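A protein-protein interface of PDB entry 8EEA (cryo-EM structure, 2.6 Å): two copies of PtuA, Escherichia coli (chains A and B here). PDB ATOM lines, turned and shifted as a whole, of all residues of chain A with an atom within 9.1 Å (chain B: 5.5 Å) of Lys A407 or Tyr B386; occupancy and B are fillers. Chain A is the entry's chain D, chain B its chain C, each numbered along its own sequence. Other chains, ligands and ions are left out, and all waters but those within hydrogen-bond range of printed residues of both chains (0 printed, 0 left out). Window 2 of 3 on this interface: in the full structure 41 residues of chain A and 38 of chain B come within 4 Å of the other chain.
The side-chain amino group (NZ) of Lys A409 is in hydrogen-bond range of the backbone carbonyl oxygen (O) of Gln A403 (3.2 Å). The backbone carbonyl oxygen of Ser B358 sits at hydrogen-bond distance from the backbone NH of Gly B387 (3.3 Å). The backbone NH of Tyr B386 is in hydrogen-bond range of the backbone carbonyl oxygen of Val B360.
No position is printed for both chains. Of the 11 pairs that touch across the chains among the printed residues, none has its exchanged pair printed and touching as well.
Of the printed residues of chain B, Val A406 touches Tyr B386 (3.9 Å) and Gly B387 (3.96 Å). Lys A407 touches one residue of chain B. Asp A411 touches none of the printed residues of chain B. Val A438 touches none of the printed residues of chain B. Of the printed residues of chain A, Ser B358 touches Pro A404. Thr B385 touches none of the printed residues of chain A. Gly B387 touches just these residues of chain A: Gln A403, Val A406 and His A444. The nearest printed residue of chain B that does not touch Lys A407 is Lys B361 (6.0 Å). The nearest residue of chain A that does not touch Tyr B386 is Leu A440 (4.04 Å).
Gln A403 touches Gly B387. Ser B358 touches Pro A404 (O to CG, 3.4 Å). Pro A404 touches Thr B359. Glu B388 touches Pro A404. CB of Val A406 touches OH of Tyr B386, 3.9 Å away. Val A406 touches Gly B387 (CG1 to CA, 3.96 Å). OE1 of Glu A408 touches CE2 of Tyr B386 (3.5 Å). OE1 of Glu B388 touches CD2 of His A444 (3.8 Å). Glu B388 touches Pro A445 (OE2 to CD, 3.4 Å).
Printed residues of chain B that touch a printed residue of chain A: Ser B358, Thr B359, Tyr B386, Gly B387 and Glu B388. Along chain B the printed residues that touch a printed residue of chain A span positions 358 to 388. Of the 19 printed residues of chain A, 7 touch a printed residue of chain B. Among the printed residues, 11 pairs touch across the chains. Among the printed residues, no Asp or Glu carboxylate lies within 4 Å of a Lys or Arg side-chain nitrogen of the other chain.
The backbone carbonyl oxygen of Gly B387 is in hydrogen-bond range of a ring nitrogen (NE2) of His A444, at 2.6 Å. The side-chain amino group of Lys A407 lies within hydrogen-bond range of the side-chain hydroxyl of Tyr B386 (3.5 Å).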
ATOM      1  N   GLN A 403      -4.443  -9.439 -27.941  1.00  0.00           N
ATOM      2  CA  GLN A 403      -5.123  -8.233 -28.399  1.00  0.00           C
ATOM      3  C   GLN A 403      -6.580  -8.271 -27.949  1.00  0.00           C
ATOM      4  O   GLN A 403      -7.317  -9.173 -28.361  1.00  0.00           O
ATOM      5  CB  GLN A 403      -5.034  -8.130 -29.919  1.00  0.00           C
ATOM      6  CG  GLN A 403      -5.892  -7.045 -30.558  1.00  0.00           C
ATOM      7  CD  GLN A 403      -5.524  -5.649 -30.098  1.00  0.00           C
ATOM      8  OE1 GLN A 403      -6.393  -4.853 -29.742  1.00  0.00           O
ATOM      9  NE2 GLN A 403      -4.233  -5.340 -30.112  1.00  0.00           N
ATOM     10  N   PRO A 404      -7.036  -7.333 -27.121  1.00  0.00           N
ATOM     11  CA  PRO A 404      -8.419  -7.390 -26.639  1.00  0.00           C
ATOM     12  C   PRO A 404      -9.418  -7.062 -27.738  1.00  0.00           C
ATOM     13  O   PRO A 404      -9.116  -6.382 -28.718  1.00  0.00           O
ATOM     14  CB  PRO A 404      -8.452  -6.341 -25.524  1.00  0.00           C
ATOM     15  CG  PRO A 404      -7.391  -5.379 -25.881  1.00  0.00           C
ATOM     16  CD  PRO A 404      -6.322  -6.154 -26.599  1.00  0.00           C
ATOM     17  N   ALA A 405     -10.641  -7.561 -27.548  1.00  0.00           N
ATOM     18  CA  ALA A 405     -11.706  -7.399 -28.539  1.00  0.00           C
ATOM     19  C   ALA A 405     -12.437  -6.077 -28.305  1.00  0.00           C
ATOM     20  O   ALA A 405     -13.601  -6.022 -27.907  1.00  0.00           O
ATOM     21  CB  ALA A 405     -12.661  -8.586 -28.488  1.00  0.00           C
ATOM     22  N   VAL A 406     -11.715  -4.990 -28.570  1.00  0.00           N
ATOM     23  CA  VAL A 406     -12.292  -3.651 -28.548  1.00  0.00           C
ATOM     24  C   VAL A 406     -13.001  -3.412 -29.873  1.00  0.00           C
ATOM     25  O   VAL A 406     -12.890  -4.220 -30.802  1.00  0.00           O
ATOM     26  CB  VAL A 406     -11.224  -2.573 -28.280  1.00  0.00           C
ATOM     27  CG1 VAL A 406     -10.681  -2.709 -26.867  1.00  0.00           C
ATOM     28  CG2 VAL A 406     -10.099  -2.647 -29.305  1.00  0.00           C
ATOM     29  N   LYS A 407     -13.750  -2.310 -29.965  1.00  0.00           N
ATOM     30  CA  LYS A 407     -14.529  -2.040 -31.170  1.00  0.00           C
ATOM     31  C   LYS A 407     -13.661  -2.027 -32.422  1.00  0.00           C
ATOM     32  O   LYS A 407     -14.111  -2.454 -33.490  1.00  0.00           O
ATOM     33  CB  LYS A 407     -15.256  -0.703 -31.037  1.00  0.00           C
ATOM     34  CG  LYS A 407     -16.029  -0.528 -29.743  1.00  0.00           C
ATOM     35  CD  LYS A 407     -17.071   0.574 -29.862  1.00  0.00           C
ATOM     36  CE  LYS A 407     -16.434   1.939 -30.087  1.00  0.00           C
ATOM     37  NZ  LYS A 407     -15.550   2.348 -28.962  1.00  0.00           N
ATOM     38  N   GLU A 408     -12.424  -1.552 -32.315  1.00  0.00           N
ATOM     39  CA  GLU A 408     -11.569  -1.334 -33.474  1.00  0.00           C
ATOM     40  C   GLU A 408     -10.767  -2.566 -33.880  1.00  0.00           C
ATOM     41  O   GLU A 408      -9.937  -2.469 -34.789  1.00  0.00           O
ATOM     42  CB  GLU A 408     -10.603  -0.175 -33.200  1.00  0.00           C
ATOM     43  CG  GLU A 408     -11.278   1.180 -33.044  1.00  0.00           C
ATOM     44  CD  GLU A 408     -11.767   1.439 -31.632  1.00  0.00           C
ATOM     45  OE1 GLU A 408     -11.595   0.560 -30.765  1.00  0.00           O
ATOM     46  OE2 GLU A 408     -12.328   2.529 -31.389  1.00  0.00           O
ATOM     47  N   LYS A 409     -10.983  -3.714 -33.237  1.00  0.00           N
ATOM     48  CA  LYS A 409     -10.165  -4.884 -33.539  1.00  0.00           C
ATOM     49  C   LYS A 409     -10.393  -5.380 -34.962  1.00  0.00           C
ATOM     50  O   LYS A 409      -9.435  -5.697 -35.677  1.00  0.00           O
ATOM     51  CB  LYS A 409     -10.449  -6.001 -32.536  1.00  0.00           C
ATOM     52  CG  LYS A 409      -9.493  -7.175 -32.662  1.00  0.00           C
ATOM     53  CD  LYS A 409      -9.709  -8.209 -31.578  1.00  0.00           C
ATOM     54  CE  LYS A 409      -8.782  -9.397 -31.763  1.00  0.00           C
ATOM     55  NZ  LYS A 409      -9.007 -10.445 -30.733  1.00  0.00           N
ATOM     56  N   ALA A 410     -11.655  -5.466 -35.394  1.00  0.00           N
ATOM     57  CA  ALA A 410     -11.943  -5.979 -36.730  1.00  0.00           C
ATOM     58  C   ALA A 410     -11.341  -5.085 -37.806  1.00  0.00           C
ATOM     59  O   ALA A 410     -10.796  -5.576 -38.804  1.00  0.00           O
ATOM     60  CB  ALA A 410     -13.452  -6.114 -36.926  1.00  0.00           C
ATOM     61  N   ASP A 411     -11.432  -3.766 -37.625  1.00  0.00           N
ATOM     62  CA  ASP A 411     -10.805  -2.850 -38.570  1.00  0.00           C
ATOM     63  C   ASP A 411      -9.296  -3.045 -38.594  1.00  0.00           C
ATOM     64  O   ASP A 411      -8.672  -2.984 -39.659  1.00  0.00           O
ATOM     65  CB  ASP A 411     -11.152  -1.407 -38.209  1.00  0.00           C
ATOM     66  CG  ASP A 411     -12.644  -1.149 -38.217  1.00  0.00           C
ATOM     67  OD1 ASP A 411     -13.383  -1.945 -38.830  1.00  0.00           O
ATOM     68  OD2 ASP A 411     -13.078  -0.147 -37.610  1.00  0.00           O
ATOM     69  N   LEU A 412      -8.689  -3.274 -37.427  1.00  0.00           N
ATOM     70  CA  LEU A 412      -7.253  -3.520 -37.378  1.00  0.00           C
ATOM     71  C   LEU A 412      -6.883  -4.781 -38.149  1.00  0.00           C
ATOM     72  O   LEU A 412      -5.897  -4.797 -38.895  1.00  0.00           O
ATOM     73  CB  LEU A 412      -6.795  -3.627 -35.923  1.00  0.00           C
ATOM     74  CG  LEU A 412      -5.288  -3.714 -35.677  1.00  0.00           C
ATOM     75  CD1 LEU A 412      -4.579  -2.466 -36.173  1.00  0.00           C
ATOM     76  CD2 LEU A 412      -5.014  -3.940 -34.200  1.00  0.00           C
ATOM     77  N   GLN A 413      -7.663  -5.851 -37.979  1.00  0.00           N
ATOM     78  CA  GLN A 413      -7.383  -7.087 -38.703  1.00  0.00           C
ATOM     79  C   GLN A 413      -7.525  -6.886 -40.206  1.00  0.00           C
ATOM     80  O   GLN A 413      -6.699  -7.376 -40.989  1.00  0.00           O
ATOM     81  CB  GLN A 413      -8.315  -8.198 -38.219  1.00  0.00           C
ATOM     82  CG  GLN A 413      -8.204  -8.482 -36.733  1.00  0.00           C
ATOM     83  CD  GLN A 413      -8.496  -9.925 -36.389  1.00  0.00           C
ATOM     84  OE1 GLN A 413      -9.472 -10.505 -36.863  1.00  0.00           O
ATOM     85  NE2 GLN A 413      -7.650 -10.516 -35.553  1.00  0.00           N
ATOM     86  N   LEU A 436      -7.730   4.442 -37.969  1.00  0.00           N
ATOM     87  CA  LEU A 436      -7.241   3.614 -36.872  1.00  0.00           C
ATOM     88  C   LEU A 436      -6.147   4.317 -36.081  1.00  0.00           C
ATOM     89  O   LEU A 436      -6.033   4.104 -34.871  1.00  0.00           O
ATOM     90  CB  LEU A 436      -6.742   2.274 -37.405  1.00  0.00           C
ATOM     91  CG  LEU A 436      -7.836   1.222 -37.585  1.00  0.00           C
ATOM     92  CD1 LEU A 436      -7.319   0.052 -38.400  1.00  0.00           C
ATOM     93  CD2 LEU A 436      -8.363   0.744 -36.241  1.00  0.00           C
ATOM     94  N   VAL A 438      -6.092   7.546 -35.447  1.00  0.00           N
ATOM     95  CA  VAL A 438      -6.779   8.447 -34.524  1.00  0.00           C
ATOM     96  C   VAL A 438      -7.529   7.663 -33.448  1.00  0.00           C
ATOM     97  O   VAL A 438      -7.644   8.129 -32.309  1.00  0.00           O
ATOM     98  CB  VAL A 438      -7.716   9.409 -35.277  1.00  0.00           C
ATOM     99  CG1 VAL A 438      -6.919  10.271 -36.243  1.00  0.00           C
ATOM    100  CG2 VAL A 438      -8.810   8.658 -36.012  1.00  0.00           C
ATOM    101  N   ALA A 439      -8.046   6.475 -33.772  1.00  0.00           N
ATOM    102  CA  ALA A 439      -8.819   5.713 -32.795  1.00  0.00           C
ATOM    103  C   ALA A 439      -7.944   5.036 -31.745  1.00  0.00           C
ATOM    104  O   ALA A 439      -8.358   4.927 -30.586  1.00  0.00           O
ATOM    105  CB  ALA A 439      -9.672   4.663 -33.506  1.00  0.00           C
ATOM    106  N   LEU A 440      -6.748   4.571 -32.120  1.00  0.00           N
ATOM    107  CA  LEU A 440      -5.870   3.844 -31.213  1.00  0.00           C
ATOM    108  C   LEU A 440      -4.545   4.540 -30.942  1.00  0.00           C
ATOM    109  O   LEU A 440      -3.809   4.095 -30.055  1.00  0.00           O
ATOM    110  CB  LEU A 440      -5.567   2.441 -31.764  1.00  0.00           C
ATOM    111  CG  LEU A 440      -6.733   1.462 -31.895  1.00  0.00           C
ATOM    112  CD1 LEU A 440      -6.419   0.410 -32.946  1.00  0.00           C
ATOM    113  CD2 LEU A 440      -7.039   0.810 -30.559  1.00  0.00           C
ATOM    114  N   GLY A 441      -4.217   5.595 -31.668  1.00  0.00           N
ATOM    115  CA  GLY A 441      -2.922   6.237 -31.508  1.00  0.00           C
ATOM    116  C   GLY A 441      -1.893   5.695 -32.479  1.00  0.00           C
ATOM    117  O   GLY A 441      -1.963   4.557 -32.940  1.00  0.00           O
ATOM    118  N   LYS A 443       1.218   5.074 -31.884  1.00  0.00           N
ATOM    119  CA  LYS A 443       2.254   4.286 -31.233  1.00  0.00           C
ATOM    120  C   LYS A 443       1.828   2.846 -30.974  1.00  0.00           C
ATOM    121  O   LYS A 443       2.534   2.122 -30.265  1.00  0.00           O
ATOM    122  CB  LYS A 443       2.667   4.949 -29.919  1.00  0.00           C
ATOM    123  CG  LYS A 443       3.229   6.351 -30.082  1.00  0.00           C
ATOM    124  CD  LYS A 443       3.495   7.001 -28.734  1.00  0.00           C
ATOM    125  CE  LYS A 443       4.275   8.297 -28.883  1.00  0.00           C
ATOM    126  NZ  LYS A 443       4.701   8.849 -27.567  1.00  0.00           N
ATOM    127  N   HIS A 444       0.701   2.416 -31.526  1.00  0.00           N
ATOM    128  CA  HIS A 444       0.269   1.037 -31.354  1.00  0.00           C
ATOM    129  C   HIS A 444       1.299   0.096 -31.977  1.00  0.00           C
ATOM    130  O   HIS A 444       1.752   0.344 -33.103  1.00  0.00           O
ATOM    131  CB  HIS A 444      -1.099   0.824 -31.998  1.00  0.00           C
ATOM    132  CG  HIS A 444      -1.881  -0.302 -31.399  1.00  0.00           C
ATOM    133  ND1 HIS A 444      -1.919  -1.562 -31.957  1.00  0.00           N
ATOM    134  CD2 HIS A 444      -2.659  -0.356 -30.294  1.00  0.00           C
ATOM    135  CE1 HIS A 444      -2.685  -2.344 -31.219  1.00  0.00           C
ATOM    136  NE2 HIS A 444      -3.147  -1.637 -30.204  1.00  0.00           N
ATOM    137  N   PRO A 445       1.702  -0.976 -31.288  1.00  0.00           N
ATOM    138  CA  PRO A 445       2.730  -1.856 -31.868  1.00  0.00           C
ATOM    139  C   PRO A 445       2.341  -2.448 -33.213  1.00  0.00           C
ATOM    140  O   PRO A 445       3.192  -2.554 -34.108  1.00  0.00           O
ATOM    141  CB  PRO A 445       2.908  -2.944 -30.797  1.00  0.00           C
ATOM    142  CG  PRO A 445       1.700  -2.859 -29.936  1.00  0.00           C
ATOM    143  CD  PRO A 445       1.268  -1.436 -29.959  1.00  0.00           C
ATOM    144  N   LEU B 357      -7.107  -3.865 -17.536  1.00  0.00           N
ATOM    145  CA  LEU B 357      -6.677  -2.518 -17.886  1.00  0.00           C
ATOM    146  C   LEU B 357      -6.569  -2.311 -19.389  1.00  0.00           C
ATOM    147  O   LEU B 357      -6.665  -1.170 -19.851  1.00  0.00           O
ATOM    148  CB  LEU B 357      -5.329  -2.215 -17.236  1.00  0.00           C
ATOM    149  CG  LEU B 357      -5.313  -2.119 -15.712  1.00  0.00           C
ATOM    150  CD1 LEU B 357      -3.921  -1.758 -15.234  1.00  0.00           C
ATOM    151  CD2 LEU B 357      -6.336  -1.116 -15.204  1.00  0.00           C
ATOM    152  N   SER B 358      -6.368  -3.371 -20.158  1.00  0.00           N
ATOM    153  CA  SER B 358      -6.223  -3.233 -21.607  1.00  0.00           C
ATOM    154  C   SER B 358      -7.526  -2.871 -22.310  1.00  0.00           C
ATOM    155  O   SER B 358      -7.526  -2.855 -23.547  1.00  0.00           O
ATOM    156  CB  SER B 358      -5.666  -4.527 -22.195  1.00  0.00           C
ATOM    157  OG  SER B 358      -6.571  -5.600 -22.014  1.00  0.00           O
ATOM    158  N   THR B 359      -8.625  -2.581 -21.609  1.00  0.00           N
ATOM    159  CA  THR B 359      -9.905  -2.304 -22.253  1.00  0.00           C
ATOM    160  C   THR B 359     -10.551  -1.025 -21.728  1.00  0.00           C
ATOM    161  O   THR B 359     -11.762  -0.847 -21.880  1.00  0.00           O
ATOM    162  CB  THR B 359     -10.863  -3.483 -22.066  1.00  0.00           C
ATOM    163  OG1 THR B 359     -10.942  -3.827 -20.678  1.00  0.00           O
ATOM    164  CG2 THR B 359     -10.383  -4.690 -22.852  1.00  0.00           C
ATOM    165  N   VAL B 360      -9.774  -0.130 -21.118  1.00  0.00           N
ATOM    166  CA  VAL B 360     -10.292   1.123 -20.586  1.00  0.00           C
ATOM    167  C   VAL B 360      -9.387   2.262 -21.033  1.00  0.00           C
ATOM    168  O   VAL B 360      -8.225   2.064 -21.392  1.00  0.00           O
ATOM    169  CB  VAL B 360     -10.403   1.106 -19.045  1.00  0.00           C
ATOM    170  CG1 VAL B 360     -11.368   0.030 -18.592  1.00  0.00           C
ATOM    171  CG2 VAL B 360      -9.042   0.899 -18.413  1.00  0.00           C
ATOM    172  N   LYS B 361      -9.943   3.470 -21.007  1.00  0.00           N
ATOM    173  CA  LYS B 361      -9.169   4.667 -21.292  1.00  0.00           C
ATOM    174  C   LYS B 361      -8.286   5.020 -20.100  1.00  0.00           C
ATOM    175  O   LYS B 361      -8.507   4.567 -18.974  1.00  0.00           O
ATOM    176  CB  LYS B 361     -10.091   5.840 -21.627  1.00  0.00           C
ATOM    177  CG  LYS B 361     -11.173   5.518 -22.645  1.00  0.00           C
ATOM    178  CD  LYS B 361     -10.602   5.416 -24.049  1.00  0.00           C
ATOM    179  CE  LYS B 361     -11.693   5.535 -25.098  1.00  0.00           C
ATOM    180  NZ  LYS B 361     -11.136   5.639 -26.473  1.00  0.00           N
ATOM    181  N   ALA B 384      -0.778   5.193 -23.124  1.00  0.00           N
ATOM    182  CA  ALA B 384      -2.105   4.741 -23.513  1.00  0.00           C
ATOM    183  C   ALA B 384      -2.310   3.285 -23.116  1.00  0.00           C
ATOM    184  O   ALA B 384      -1.358   2.505 -23.024  1.00  0.00           O
ATOM    185  CB  ALA B 384      -2.313   4.901 -25.018  1.00  0.00           C
ATOM    186  N   THR B 385      -3.572   2.925 -22.880  1.00  0.00           N
ATOM    187  CA  THR B 385      -3.928   1.578 -22.456  1.00  0.00           C
ATOM    188  C   THR B 385      -5.128   0.994 -23.189  1.00  0.00           C
ATOM    189  O   THR B 385      -5.383  -0.206 -23.048  1.00  0.00           O
ATOM    190  CB  THR B 385      -4.218   1.549 -20.949  1.00  0.00           C
ATOM    191  OG1 THR B 385      -5.282   2.459 -20.644  1.00  0.00           O
ATOM    192  CG2 THR B 385      -2.986   1.942 -20.156  1.00  0.00           C
ATOM    193  N   TYR B 386      -5.867   1.789 -23.961  1.00  0.00           N
ATOM    194  CA  TYR B 386      -7.052   1.294 -24.648  1.00  0.00           C
ATOM    195  C   TYR B 386      -6.651   0.486 -25.875  1.00  0.00           C
ATOM    196  O   TYR B 386      -5.852   0.943 -26.697  1.00  0.00           O
ATOM    197  CB  TYR B 386      -7.952   2.458 -25.054  1.00  0.00           C
ATOM    198  CG  TYR B 386      -9.257   2.029 -25.680  1.00  0.00           C
ATOM    199  CD1 TYR B 386     -10.261   1.460 -24.913  1.00  0.00           C
ATOM    200  CD2 TYR B 386      -9.487   2.197 -27.039  1.00  0.00           C
ATOM    201  CE1 TYR B 386     -11.455   1.065 -25.478  1.00  0.00           C
ATOM    202  CE2 TYR B 386     -10.679   1.804 -27.613  1.00  0.00           C
ATOM    203  CZ  TYR B 386     -11.659   1.240 -26.828  1.00  0.00           C
ATOM    204  OH  TYR B 386     -12.850   0.847 -27.393  1.00  0.00           O
ATOM    205  N   GLY B 387      -7.211  -0.715 -25.998  1.00  0.00           N
ATOM    206  CA  GLY B 387      -6.897  -1.564 -27.134  1.00  0.00           C
ATOM    207  C   GLY B 387      -5.427  -1.891 -27.248  1.00  0.00           C
ATOM    208  O   GLY B 387      -4.896  -1.959 -28.362  1.00  0.00           O
ATOM    209  N   GLU B 388      -4.753  -2.105 -26.123  1.00  0.00           N
ATOM    210  CA  GLU B 388      -3.322  -2.320 -26.073  1.00  0.00           C
ATOM    211  C   GLU B 388      -3.014  -3.765 -25.694  1.00  0.00           C
ATOM    212  O   GLU B 388      -3.747  -4.354 -24.892  1.00  0.00           O
ATOM    213  CB  GLU B 388      -2.682  -1.376 -25.048  1.00  0.00           C
ATOM    214  CG  GLU B 388      -1.234  -1.023 -25.323  1.00  0.00           C
ATOM    215  CD  GLU B 388      -1.082  -0.049 -26.473  1.00  0.00           C
ATOM    216  OE1 GLU B 388      -2.004   0.763 -26.693  1.00  0.00           O
ATOM    217  OE2 GLU B 388      -0.038  -0.093 -27.158  1.00  0.00           O
